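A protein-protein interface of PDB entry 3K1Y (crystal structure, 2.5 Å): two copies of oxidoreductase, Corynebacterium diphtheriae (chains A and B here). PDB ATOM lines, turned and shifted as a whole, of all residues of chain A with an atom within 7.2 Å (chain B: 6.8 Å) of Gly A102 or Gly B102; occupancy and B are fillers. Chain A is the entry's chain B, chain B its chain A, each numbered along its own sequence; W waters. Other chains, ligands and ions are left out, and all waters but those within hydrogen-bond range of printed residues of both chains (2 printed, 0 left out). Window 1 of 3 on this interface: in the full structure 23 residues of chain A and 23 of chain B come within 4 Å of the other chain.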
ATOM      1  N   LEU A  56      17.382  21.679 -33.072  1.00  0.00           N
ATOM      2  CA  LEU A  56      16.909  20.296 -33.056  1.00  0.00           C
ATOM      3  C   LEU A  56      15.674  20.052 -33.901  1.00  0.00           C
ATOM      4  O   LEU A  56      15.525  18.989 -34.486  1.00  0.00           O
ATOM      5  CB  LEU A  56      16.644  19.833 -31.624  1.00  0.00           C
ATOM      6  CG  LEU A  56      17.879  19.663 -30.735  1.00  0.00           C
ATOM      7  CD1 LEU A  56      17.477  18.951 -29.437  1.00  0.00           C
ATOM      8  CD2 LEU A  56      18.948  18.867 -31.476  1.00  0.00           C
ATOM      9  N   MET A  67      17.126   6.242 -34.417  1.00  0.00           N
ATOM     10  CA  MET A  67      16.386   5.456 -33.435  1.00  0.00           C
ATOM     11  C   MET A  67      16.014   4.085 -33.988  1.00  0.00           C
ATOM     12  O   MET A  67      16.117   3.080 -33.292  1.00  0.00           O
ATOM     13  CB  MET A  67      15.119   6.194 -32.992  1.00  0.00           C
ATOM     14  CG  MET A  67      15.359   7.452 -32.152  1.00  0.00           C
ATOM     15  SD  MET A  67      16.140   7.136 -30.396  1.00  0.00           S
ATOM     16  CE  MET A  67      14.565   6.517 -29.470  1.00  0.00           C
ATOM     17  N   THR A  93      16.378  24.607 -23.666  1.00  0.00           N
ATOM     18  CA  THR A  93      15.186  23.845 -23.950  1.00  0.00           C
ATOM     19  C   THR A  93      13.909  24.406 -23.366  1.00  0.00           C
ATOM     20  O   THR A  93      13.921  25.078 -22.334  1.00  0.00           O
ATOM     21  CB  THR A  93      15.320  22.417 -23.408  1.00  0.00           C
ATOM     22  OG1 THR A  93      14.105  21.697 -23.653  1.00  0.00           O
ATOM     23  CG2 THR A  93      15.581  22.451 -21.896  1.00  0.00           C
ATOM     24  N   PHE A  96       8.326  20.869 -21.416  1.00  0.00           N
ATOM     25  CA  PHE A  96       7.114  20.085 -21.677  1.00  0.00           C
ATOM     26  C   PHE A  96       6.994  19.069 -20.541  1.00  0.00           C
ATOM     27  O   PHE A  96       7.946  18.359 -20.232  1.00  0.00           O
ATOM     28  CB  PHE A  96       7.192  19.323 -23.005  1.00  0.00           C
ATOM     29  CG  PHE A  96       7.331  20.193 -24.228  1.00  0.00           C
ATOM     30  CD1 PHE A  96       7.127  21.569 -24.169  1.00  0.00           C
ATOM     31  CD2 PHE A  96       7.635  19.615 -25.462  1.00  0.00           C
ATOM     32  CE1 PHE A  96       7.219  22.359 -25.325  1.00  0.00           C
ATOM     33  CE2 PHE A  96       7.732  20.397 -26.626  1.00  0.00           C
ATOM     34  CZ  PHE A  96       7.522  21.769 -26.556  1.00  0.00           C
ATOM     35  N   SER A  99       9.710  19.326 -17.354  1.00  0.00           N
ATOM     36  CA  SER A  99      11.071  18.832 -17.492  1.00  0.00           C
ATOM     37  C   SER A  99      11.519  19.139 -18.921  1.00  0.00           C
ATOM     38  O   SER A  99      10.759  19.724 -19.697  1.00  0.00           O
ATOM     39  CB  SER A  99      11.105  17.328 -17.241  1.00  0.00           C
ATOM     40  OG  SER A  99      12.389  16.799 -17.524  1.00  0.00           O
ATOM     41  N   TYR A 100      12.738  18.749 -19.282  1.00  0.00           N
ATOM     42  CA  TYR A 100      13.185  19.035 -20.629  1.00  0.00           C
ATOM     43  C   TYR A 100      12.417  18.221 -21.671  1.00  0.00           C
ATOM     44  O   TYR A 100      11.760  17.216 -21.345  1.00  0.00           O
ATOM     45  CB  TYR A 100      14.697  18.814 -20.776  1.00  0.00           C
ATOM     46  CG  TYR A 100      15.228  17.472 -20.300  1.00  0.00           C
ATOM     47  CD1 TYR A 100      14.603  16.275 -20.653  1.00  0.00           C
ATOM     48  CD2 TYR A 100      16.392  17.406 -19.533  1.00  0.00           C
ATOM     49  CE1 TYR A 100      15.125  15.054 -20.255  1.00  0.00           C
ATOM     50  CE2 TYR A 100      16.920  16.192 -19.135  1.00  0.00           C
ATOM     51  CZ  TYR A 100      16.287  15.021 -19.496  1.00  0.00           C
ATOM     52  OH  TYR A 100      16.827  13.826 -19.091  1.00  0.00           O
ATOM     53  N   THR A 101      12.503  18.676 -22.919  1.00  0.00           N
ATOM     54  CA  THR A 101      11.827  18.063 -24.060  1.00  0.00           C
ATOM     55  C   THR A 101      12.324  16.672 -24.460  1.00  0.00           C
ATOM     56  O   THR A 101      13.511  16.348 -24.338  1.00  0.00           O
ATOM     57  CB  THR A 101      11.931  18.996 -25.286  1.00  0.00           C
ATOM     58  OG1 THR A 101      10.672  19.636 -25.513  1.00  0.00           O
ATOM     59  CG2 THR A 101      12.334  18.232 -26.507  1.00  0.00           C
ATOM     60  N   GLY A 102      11.400  15.857 -24.954  1.00  0.00           N
ATOM     61  CA  GLY A 102      11.760  14.523 -25.386  1.00  0.00           C
ATOM     62  C   GLY A 102      12.789  14.618 -26.494  1.00  0.00           C
ATOM     63  O   GLY A 102      13.826  13.949 -26.464  1.00  0.00           O
ATOM     64  N   LEU A 103      12.501  15.466 -27.475  1.00  0.00           N
ATOM     65  CA  LEU A 103      13.405  15.672 -28.594  1.00  0.00           C
ATOM     66  C   LEU A 103      14.776  16.087 -28.049  1.00  0.00           C
ATOM     67  O   LEU A 103      15.811  15.599 -28.503  1.00  0.00           O
ATOM     68  CB  LEU A 103      12.844  16.749 -29.524  1.00  0.00           C
ATOM     69  CG  LEU A 103      13.736  17.164 -30.699  1.00  0.00           C
ATOM     70  CD1 LEU A 103      13.959  15.981 -31.631  1.00  0.00           C
ATOM     71  CD2 LEU A 103      13.094  18.320 -31.440  1.00  0.00           C
ATOM     72  N   PHE A 104      14.772  16.980 -27.063  1.00  0.00           N
ATOM     73  CA  PHE A 104      16.007  17.454 -26.449  1.00  0.00           C
ATOM     74  C   PHE A 104      16.827  16.271 -25.936  1.00  0.00           C
ATOM     75  O   PHE A 104      18.007  16.138 -26.262  1.00  0.00           O
ATOM     76  CB  PHE A 104      15.699  18.394 -25.287  1.00  0.00           C
ATOM     77  CG  PHE A 104      16.927  19.001 -24.647  1.00  0.00           C
ATOM     78  CD1 PHE A 104      17.528  20.131 -25.193  1.00  0.00           C
ATOM     79  CD2 PHE A 104      17.488  18.432 -23.500  1.00  0.00           C
ATOM     80  CE1 PHE A 104      18.662  20.686 -24.610  1.00  0.00           C
ATOM     81  CE2 PHE A 104      18.628  18.981 -22.905  1.00  0.00           C
ATOM     82  CZ  PHE A 104      19.217  20.108 -23.458  1.00  0.00           C
ATOM     83  N   LYS A 105      16.196  15.411 -25.139  1.00  0.00           N
ATOM     84  CA  LYS A 105      16.869  14.251 -24.574  1.00  0.00           C
ATOM     85  C   LYS A 105      17.317  13.241 -25.632  1.00  0.00           C
ATOM     86  O   LYS A 105      18.279  12.491 -25.414  1.00  0.00           O
ATOM     87  CB  LYS A 105      15.946  13.568 -23.566  1.00  0.00           C
ATOM     88  CG  LYS A 105      16.551  12.368 -22.851  1.00  0.00           C
ATOM     89  CD  LYS A 105      17.805  12.741 -22.074  1.00  0.00           C
ATOM     90  CE  LYS A 105      18.210  11.619 -21.115  1.00  0.00           C
ATOM     91  NZ  LYS A 105      18.235  10.261 -21.774  1.00  0.00           N
ATOM     92  N   MET A 106      16.628  13.231 -26.771  1.00  0.00           N
ATOM     93  CA  MET A 106      16.943  12.308 -27.857  1.00  0.00           C
ATOM     94  C   MET A 106      18.280  12.605 -28.534  1.00  0.00           C
ATOM     95  O   MET A 106      19.013  11.691 -28.899  1.00  0.00           O
ATOM     96  CB  MET A 106      15.828  12.325 -28.902  1.00  0.00           C
ATOM     97  CG  MET A 106      15.895  11.152 -29.854  1.00  0.00           C
ATOM     98  SD  MET A 106      14.297  10.942 -30.909  1.00  0.00           S
ATOM     99  CE  MET A 106      13.038  10.554 -29.495  1.00  0.00           C
ATOM    100  N   PHE A 107      18.584  13.884 -28.716  1.00  0.00           N
ATOM    101  CA  PHE A 107      19.840  14.297 -29.323  1.00  0.00           C
ATOM    102  C   PHE A 107      20.978  13.827 -28.419  1.00  0.00           C
ATOM    103  O   PHE A 107      22.023  13.384 -28.899  1.00  0.00           O
ATOM    104  CB  PHE A 107      19.900  15.824 -29.454  1.00  0.00           C
ATOM    105  CG  PHE A 107      21.211  16.336 -29.993  1.00  0.00           C
ATOM    106  CD1 PHE A 107      21.483  16.306 -31.359  1.00  0.00           C
ATOM    107  CD2 PHE A 107      22.186  16.832 -29.133  1.00  0.00           C
ATOM    108  CE1 PHE A 107      22.704  16.764 -31.855  1.00  0.00           C
ATOM    109  CE2 PHE A 107      23.414  17.293 -29.622  1.00  0.00           C
ATOM    110  CZ  PHE A 107      23.674  17.260 -30.979  1.00  0.00           C
ATOM    111  N   PHE A 108      20.779  13.926 -27.107  1.00  0.00           N
ATOM    112  CA  PHE A 108      21.811  13.501 -26.168  1.00  0.00           C
ATOM    113  C   PHE A 108      21.926  11.980 -26.019  1.00  0.00           C
ATOM    114  O   PHE A 108      23.013  11.462 -25.724  1.00  0.00           O
ATOM    115  CB  PHE A 108      21.579  14.159 -24.809  1.00  0.00           C
ATOM    116  CG  PHE A 108      21.838  15.640 -24.816  1.00  0.00           C
ATOM    117  CD1 PHE A 108      23.146  16.134 -24.722  1.00  0.00           C
ATOM    118  CD2 PHE A 108      20.786  16.544 -24.969  1.00  0.00           C
ATOM    119  CE1 PHE A 108      23.400  17.508 -24.780  1.00  0.00           C
ATOM    120  CE2 PHE A 108      21.027  17.917 -25.033  1.00  0.00           C
ATOM    121  CZ  PHE A 108      22.336  18.403 -24.938  1.00  0.00           C
ATOM    122  N   ASP A 109      20.819  11.269 -26.229  1.00  0.00           N
ATOM    123  CA  ASP A 109      20.827   9.816 -26.111  1.00  0.00           C
ATOM    124  C   ASP A 109      21.646   9.196 -27.220  1.00  0.00           C
ATOM    125  O   ASP A 109      22.203   8.107 -27.074  1.00  0.00           O
ATOM    126  CB  ASP A 109      19.411   9.244 -26.197  1.00  0.00           C
ATOM    127  CG  ASP A 109      18.573   9.590 -25.002  1.00  0.00           C
ATOM    128  OD1 ASP A 109      19.139  10.045 -23.988  1.00  0.00           O
ATOM    129  OD2 ASP A 109      17.345   9.398 -25.077  1.00  0.00           O
ATOM    130  N   MET B  67       5.223  15.514 -34.021  1.00  0.00           N
ATOM    131  CA  MET B  67       6.224  16.492 -33.600  1.00  0.00           C
ATOM    132  C   MET B  67       6.268  17.631 -34.609  1.00  0.00           C
ATOM    133  O   MET B  67       6.106  18.799 -34.260  1.00  0.00           O
ATOM    134  CB  MET B  67       7.612  15.848 -33.515  1.00  0.00           C
ATOM    135  CG  MET B  67       7.898  15.113 -32.216  1.00  0.00           C
ATOM    136  SD  MET B  67       7.879  16.287 -30.676  1.00  0.00           S
ATOM    137  CE  MET B  67       9.548  17.208 -30.992  1.00  0.00           C
ATOM    138  N   THR B  93      11.037   1.854 -19.206  1.00  0.00           N
ATOM    139  CA  THR B  93      12.005   2.545 -20.029  1.00  0.00           C
ATOM    140  C   THR B  93      13.430   2.100 -19.779  1.00  0.00           C
ATOM    141  O   THR B  93      13.811   1.797 -18.651  1.00  0.00           O
ATOM    142  CB  THR B  93      11.974   4.083 -19.789  1.00  0.00           C
ATOM    143  OG1 THR B  93      12.903   4.727 -20.672  1.00  0.00           O
ATOM    144  CG2 THR B  93      12.391   4.410 -18.349  1.00  0.00           C
ATOM    145  N   PHE B  96      18.916   5.765 -20.586  1.00  0.00           N
ATOM    146  CA  PHE B  96      19.874   6.378 -21.495  1.00  0.00           C
ATOM    147  C   PHE B  96      20.348   7.654 -20.824  1.00  0.00           C
ATOM    148  O   PHE B  96      19.542   8.422 -20.301  1.00  0.00           O
ATOM    149  CB  PHE B  96      19.217   6.717 -22.845  1.00  0.00           C
ATOM    150  CG  PHE B  96      18.856   5.515 -23.683  1.00  0.00           C
ATOM    151  CD1 PHE B  96      19.009   4.222 -23.195  1.00  0.00           C
ATOM    152  CD2 PHE B  96      18.321   5.688 -24.959  1.00  0.00           C
ATOM    153  CE1 PHE B  96      18.633   3.119 -23.959  1.00  0.00           C
ATOM    154  CE2 PHE B  96      17.942   4.593 -25.732  1.00  0.00           C
ATOM    155  CZ  PHE B  96      18.097   3.306 -25.229  1.00  0.00           C
ATOM    156  N   SER B  99      18.804   8.516 -17.308  1.00  0.00           N
ATOM    157  CA  SER B  99      17.411   8.878 -17.100  1.00  0.00           C
ATOM    158  C   SER B  99      16.534   8.185 -18.130  1.00  0.00           C
ATOM    159  O   SER B  99      17.004   7.318 -18.870  1.00  0.00           O
ATOM    160  CB  SER B  99      17.241  10.395 -17.181  1.00  0.00           C
ATOM    161  OG  SER B  99      15.902  10.763 -16.906  1.00  0.00           O
ATOM    162  N   TYR B 100      15.256   8.544 -18.175  1.00  0.00           N
ATOM    163  CA  TYR B 100      14.361   7.920 -19.140  1.00  0.00           C
ATOM    164  C   TYR B 100      14.743   8.337 -20.551  1.00  0.00           C
ATOM    165  O   TYR B 100      15.403   9.356 -20.749  1.00  0.00           O
ATOM    166  CB  TYR B 100      12.903   8.267 -18.838  1.00  0.00           C
ATOM    167  CG  TYR B 100      12.585   9.734 -18.703  1.00  0.00           C
ATOM    168  CD1 TYR B 100      12.875  10.636 -19.730  1.00  0.00           C
ATOM    169  CD2 TYR B 100      11.915  10.210 -17.579  1.00  0.00           C
ATOM    170  CE1 TYR B 100      12.494  11.979 -19.642  1.00  0.00           C
ATOM    171  CE2 TYR B 100      11.534  11.543 -17.478  1.00  0.00           C
ATOM    172  CZ  TYR B 100      11.822  12.420 -18.511  1.00  0.00           C
ATOM    173  OH  TYR B 100      11.413  13.729 -18.416  1.00  0.00           O
ATOM    174  N   THR B 101      14.341   7.538 -21.528  1.00  0.00           N
ATOM    175  CA  THR B 101      14.677   7.802 -22.925  1.00  0.00           C
ATOM    176  C   THR B 101      13.969   9.018 -23.513  1.00  0.00           C
ATOM    177  O   THR B 101      12.856   9.359 -23.113  1.00  0.00           O
ATOM    178  CB  THR B 101      14.347   6.577 -23.804  1.00  0.00           C
ATOM    179  OG1 THR B 101      15.115   5.448 -23.371  1.00  0.00           O
ATOM    180  CG2 THR B 101      14.683   6.859 -25.234  1.00  0.00           C
ATOM    181  N   GLY B 102      14.624   9.671 -24.467  1.00  0.00           N
ATOM    182  CA  GLY B 102      14.017  10.819 -25.104  1.00  0.00           C
ATOM    183  C   GLY B 102      12.738  10.364 -25.784  1.00  0.00           C
ATOM    184  O   GLY B 102      11.728  11.070 -25.755  1.00  0.00           O
ATOM    185  N   LEU B 103      12.776   9.173 -26.381  1.00  0.00           N
ATOM    186  CA  LEU B 103      11.614   8.624 -27.074  1.00  0.00           C
ATOM    187  C   LEU B 103      10.468   8.377 -26.087  1.00  0.00           C
ATOM    188  O   LEU B 103       9.297   8.614 -26.395  1.00  0.00           O
ATOM    189  CB  LEU B 103      11.984   7.323 -27.787  1.00  0.00           C
ATOM    190  CG  LEU B 103      10.851   6.591 -28.524  1.00  0.00           C
ATOM    191  CD1 LEU B 103      10.368   7.435 -29.700  1.00  0.00           C
ATOM    192  CD2 LEU B 103      11.351   5.220 -29.006  1.00  0.00           C
ATOM    193  N   PHE B 104      10.818   7.888 -24.904  1.00  0.00           N
ATOM    194  CA  PHE B 104       9.842   7.640 -23.863  1.00  0.00           C
ATOM    195  C   PHE B 104       9.233   9.000 -23.540  1.00  0.00           C
ATOM    196  O   PHE B 104       8.008   9.151 -23.475  1.00  0.00           O
ATOM    197  CB  PHE B 104      10.556   7.070 -22.633  1.00  0.00           C
ATOM    198  CG  PHE B 104       9.675   6.898 -21.419  1.00  0.00           C
ATOM    199  CD1 PHE B 104       8.964   5.720 -21.221  1.00  0.00           C
ATOM    200  CD2 PHE B 104       9.615   7.895 -20.437  1.00  0.00           C
ATOM    201  CE1 PHE B 104       8.208   5.524 -20.059  1.00  0.00           C
ATOM    202  CE2 PHE B 104       8.867   7.714 -19.277  1.00  0.00           C
ATOM    203  CZ  PHE B 104       8.160   6.519 -19.084  1.00  0.00           C
ATOM    204  N   LYS B 105      10.097   9.993 -23.356  1.00  0.00           N
ATOM    205  CA  LYS B 105       9.639  11.336 -23.014  1.00  0.00           C
ATOM    206  C   LYS B 105       8.759  11.930 -24.106  1.00  0.00           C
ATOM    207  O   LYS B 105       7.743  12.572 -23.821  1.00  0.00           O
ATOM    208  CB  LYS B 105      10.833  12.264 -22.758  1.00  0.00           C
ATOM    209  CG  LYS B 105      10.450  13.679 -22.301  1.00  0.00           C
ATOM    210  CD  LYS B 105       9.551  13.632 -21.058  1.00  0.00           C
ATOM    211  CE  LYS B 105       9.561  14.953 -20.291  1.00  0.00           C
ATOM    212  NZ  LYS B 105       9.142  16.134 -21.095  1.00  0.00           N
ATOM    213  N   MET B 106       9.147  11.712 -25.354  1.00  0.00           N
ATOM    214  CA  MET B 106       8.395  12.247 -26.470  1.00  0.00           C
ATOM    215  C   MET B 106       6.935  11.832 -26.416  1.00  0.00           C
ATOM    216  O   MET B 106       6.041  12.665 -26.552  1.00  0.00           O
ATOM    217  CB  MET B 106       9.018  11.790 -27.780  1.00  0.00           C
ATOM    218  CG  MET B 106       8.491  12.522 -28.993  1.00  0.00           C
ATOM    219  SD  MET B 106       9.532  12.049 -30.532  1.00  0.00           S
ATOM    220  CE  MET B 106      11.096  13.153 -30.182  1.00  0.00           C
ATOM    221  N   PHE B 107       6.691  10.542 -26.212  1.00  0.00           N
ATOM    222  CA  PHE B 107       5.326  10.035 -26.145  1.00  0.00           C
ATOM    223  C   PHE B 107       4.510  10.871 -25.163  1.00  0.00           C
ATOM    224  O   PHE B 107       3.476  11.439 -25.528  1.00  0.00           O
ATOM    225  CB  PHE B 107       5.311   8.564 -25.713  1.00  0.00           C
ATOM    226  CG  PHE B 107       3.922   7.973 -25.611  1.00  0.00           C
ATOM    227  CD1 PHE B 107       3.186   7.681 -26.758  1.00  0.00           C
ATOM    228  CD2 PHE B 107       3.347   7.724 -24.366  1.00  0.00           C
ATOM    229  CE1 PHE B 107       1.893   7.143 -26.666  1.00  0.00           C
ATOM    230  CE2 PHE B 107       2.062   7.191 -24.261  1.00  0.00           C
ATOM    231  CZ  PHE B 107       1.333   6.899 -25.419  1.00  0.00           C
ATOM    232  N   ASP B 109       5.101  13.797 -23.938  1.00  0.00           N
ATOM    233  CA  ASP B 109       4.968  15.176 -24.401  1.00  0.00           C
ATOM    234  C   ASP B 109       3.761  15.319 -25.332  1.00  0.00           C
ATOM    235  O   ASP B 109       3.060  16.330 -25.319  1.00  0.00           O
ATOM    236  CB  ASP B 109       6.215  15.630 -25.172  1.00  0.00           C
ATOM    237  CG  ASP B 109       7.463  15.663 -24.313  1.00  0.00           C
ATOM    238  OD1 ASP B 109       7.349  15.847 -23.083  1.00  0.00           O
ATOM    239  OD2 ASP B 109       8.564  15.526 -24.879  1.00  0.00           O
HETATM  240  O   HOH W   1       9.788  16.180 -27.721  1.00  0.00           O
HETATM  241  O   HOH W   2      15.865   8.802 -27.071  1.00  0.00           O
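The backbone NH (N) of Gly B102 sits at hydrogen-bond distance from the side-chain carboxylate (OD2) of Asp A109 (2.8 Å).
The side-chain hydroxyl (OH) of Tyr B100 is in hydrogen-bond range of the side-chain hydroxyl (OG) of Ser A99 (3.3 Å).
O of Phe A96 is in hydrogen-bond range of NZ of Lys B105, 2.7 Å away.
N of Gly A102 is in hydrogen-bond range of OD2 of Asp B109 (2.9 Å).
The backbone carbonyl oxygen (O) of Tyr B100 lies within hydrogen-bond range of the side-chain amino group (NZ) of Lys A105, at 3.1 Å.
The side-chain amino group (NZ) of Lys B105 lies within hydrogen-bond range of the backbone carbonyl oxygen (O) of Tyr A100, at 2.8 Å.
The backbone carbonyl oxygen (O) of Phe B96 sits at hydrogen-bond distance from the side-chain amino group (NZ) of Lys A105.
OD1 of Asp B109 lies within salt-bridge range of NZ of Lys B105 (2.7 Å).
The side-chain hydroxyl (OG1) of Thr B93 is in hydrogen-bond range of the backbone NH (N) of Thr B101, 3.3 Å away.
The side-chain hydroxyl (OG1) of Thr A93 lies within hydrogen-bond range of the backbone NH (N) of Thr A101 (3.5 Å).
The side-chain amino group (NZ) of Lys A105 lies within salt-bridge range of the side-chain carboxylate (OD1) of Asp A109, at 2.4 Å.
Among the printed residues, pairs that only touch across the chains: Met A67 with Leu B103 (3.2 Å), Phe A96 with Asp B109 (3.5 Å), Tyr A100 with Ser B99 (3.9 Å), Thr A101 with Asp B109 (3.95 Å), Gly A102 with Gly B102 (3.4 Å), Gly A102 with Lys B105 (3.5 Å), Gly A102 with Met B106 (3.8 Å), Leu A103 with Met B67 (3.6 Å), Leu A103 with Met B106 (3.8 Å), Lys A105 with Gly B102 (3.7 Å), Met A106 with Gly B102 (3.7 Å), Met A106 with Leu B103 (3.4 Å), Met A106 with Met B106 (3.3 Å), Asp A109 with Phe B96 (3.5 Å) and Asp A109 with Thr B101 (3.7 Å).
Of chain B, only Gly B102, Lys B105, Met B106 and Asp B109 come within 4 Å of Gly A102.
Of chain A, only Gly A102, Lys A105, Met A106 and Asp A109 come within 4 Å of Gly B102.
Of the printed residues of chain B, Thr A101 touches Asp B109.
Printed residues of chain B within 4 Å of Leu A103: Met B67 and Met B106.
Printed residues of chain B within 4 Å of Lys A105: Phe B96 (2.7 Å), Tyr B100 (3.1 Å) and Gly B102 (3.7 Å).
Thr B93 touches none of the printed residues of chain A.
Phe B104 touches none of the printed residues of chain A.
The nearest residue of chain B that does not touch Gly A102 is Leu B103 (4.9 Å).
Of the 13 printed residues of chain B, 10 touch a printed residue of chain A.
Hydrophobic or aromatic side chains of chain B that line the printed part of chain A: Met B67, Phe B96, Tyr B100, Leu B103 and Met B106.
Along chain A the printed residues that touch a printed residue of chain B span positions 67 to 109.
Gly B102 touches its own counterpart, Gly A102.
Gly A102 touches Lys B105, and with the chains exchanged Lys A105 touches Gly B102.
Gly A102 touches Met B106, and with the chains exchanged Met A106 touches Gly B102.
Met A106 touches its own counterpart, Met B106.
13 positions are printed for both chains.
Of the 22 pairs that touch across the chains among the printed residues, 22 have their exchanged pair printed and touching as well.
Water W2 lies within hydrogen-bond range of the side-chain carboxylate of Asp A109, the backbone NH of Gly B102, the backbone NH of Leu B103 and the side-chain sulfur of Met A67.
Water W1 lies within hydrogen-bond range of N of Leu A103 (2.8 Å), OD2 of Asp B109 (3.2 Å), N of Gly A102 (3.2 Å) and SD of Met B67 (3.5 Å).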
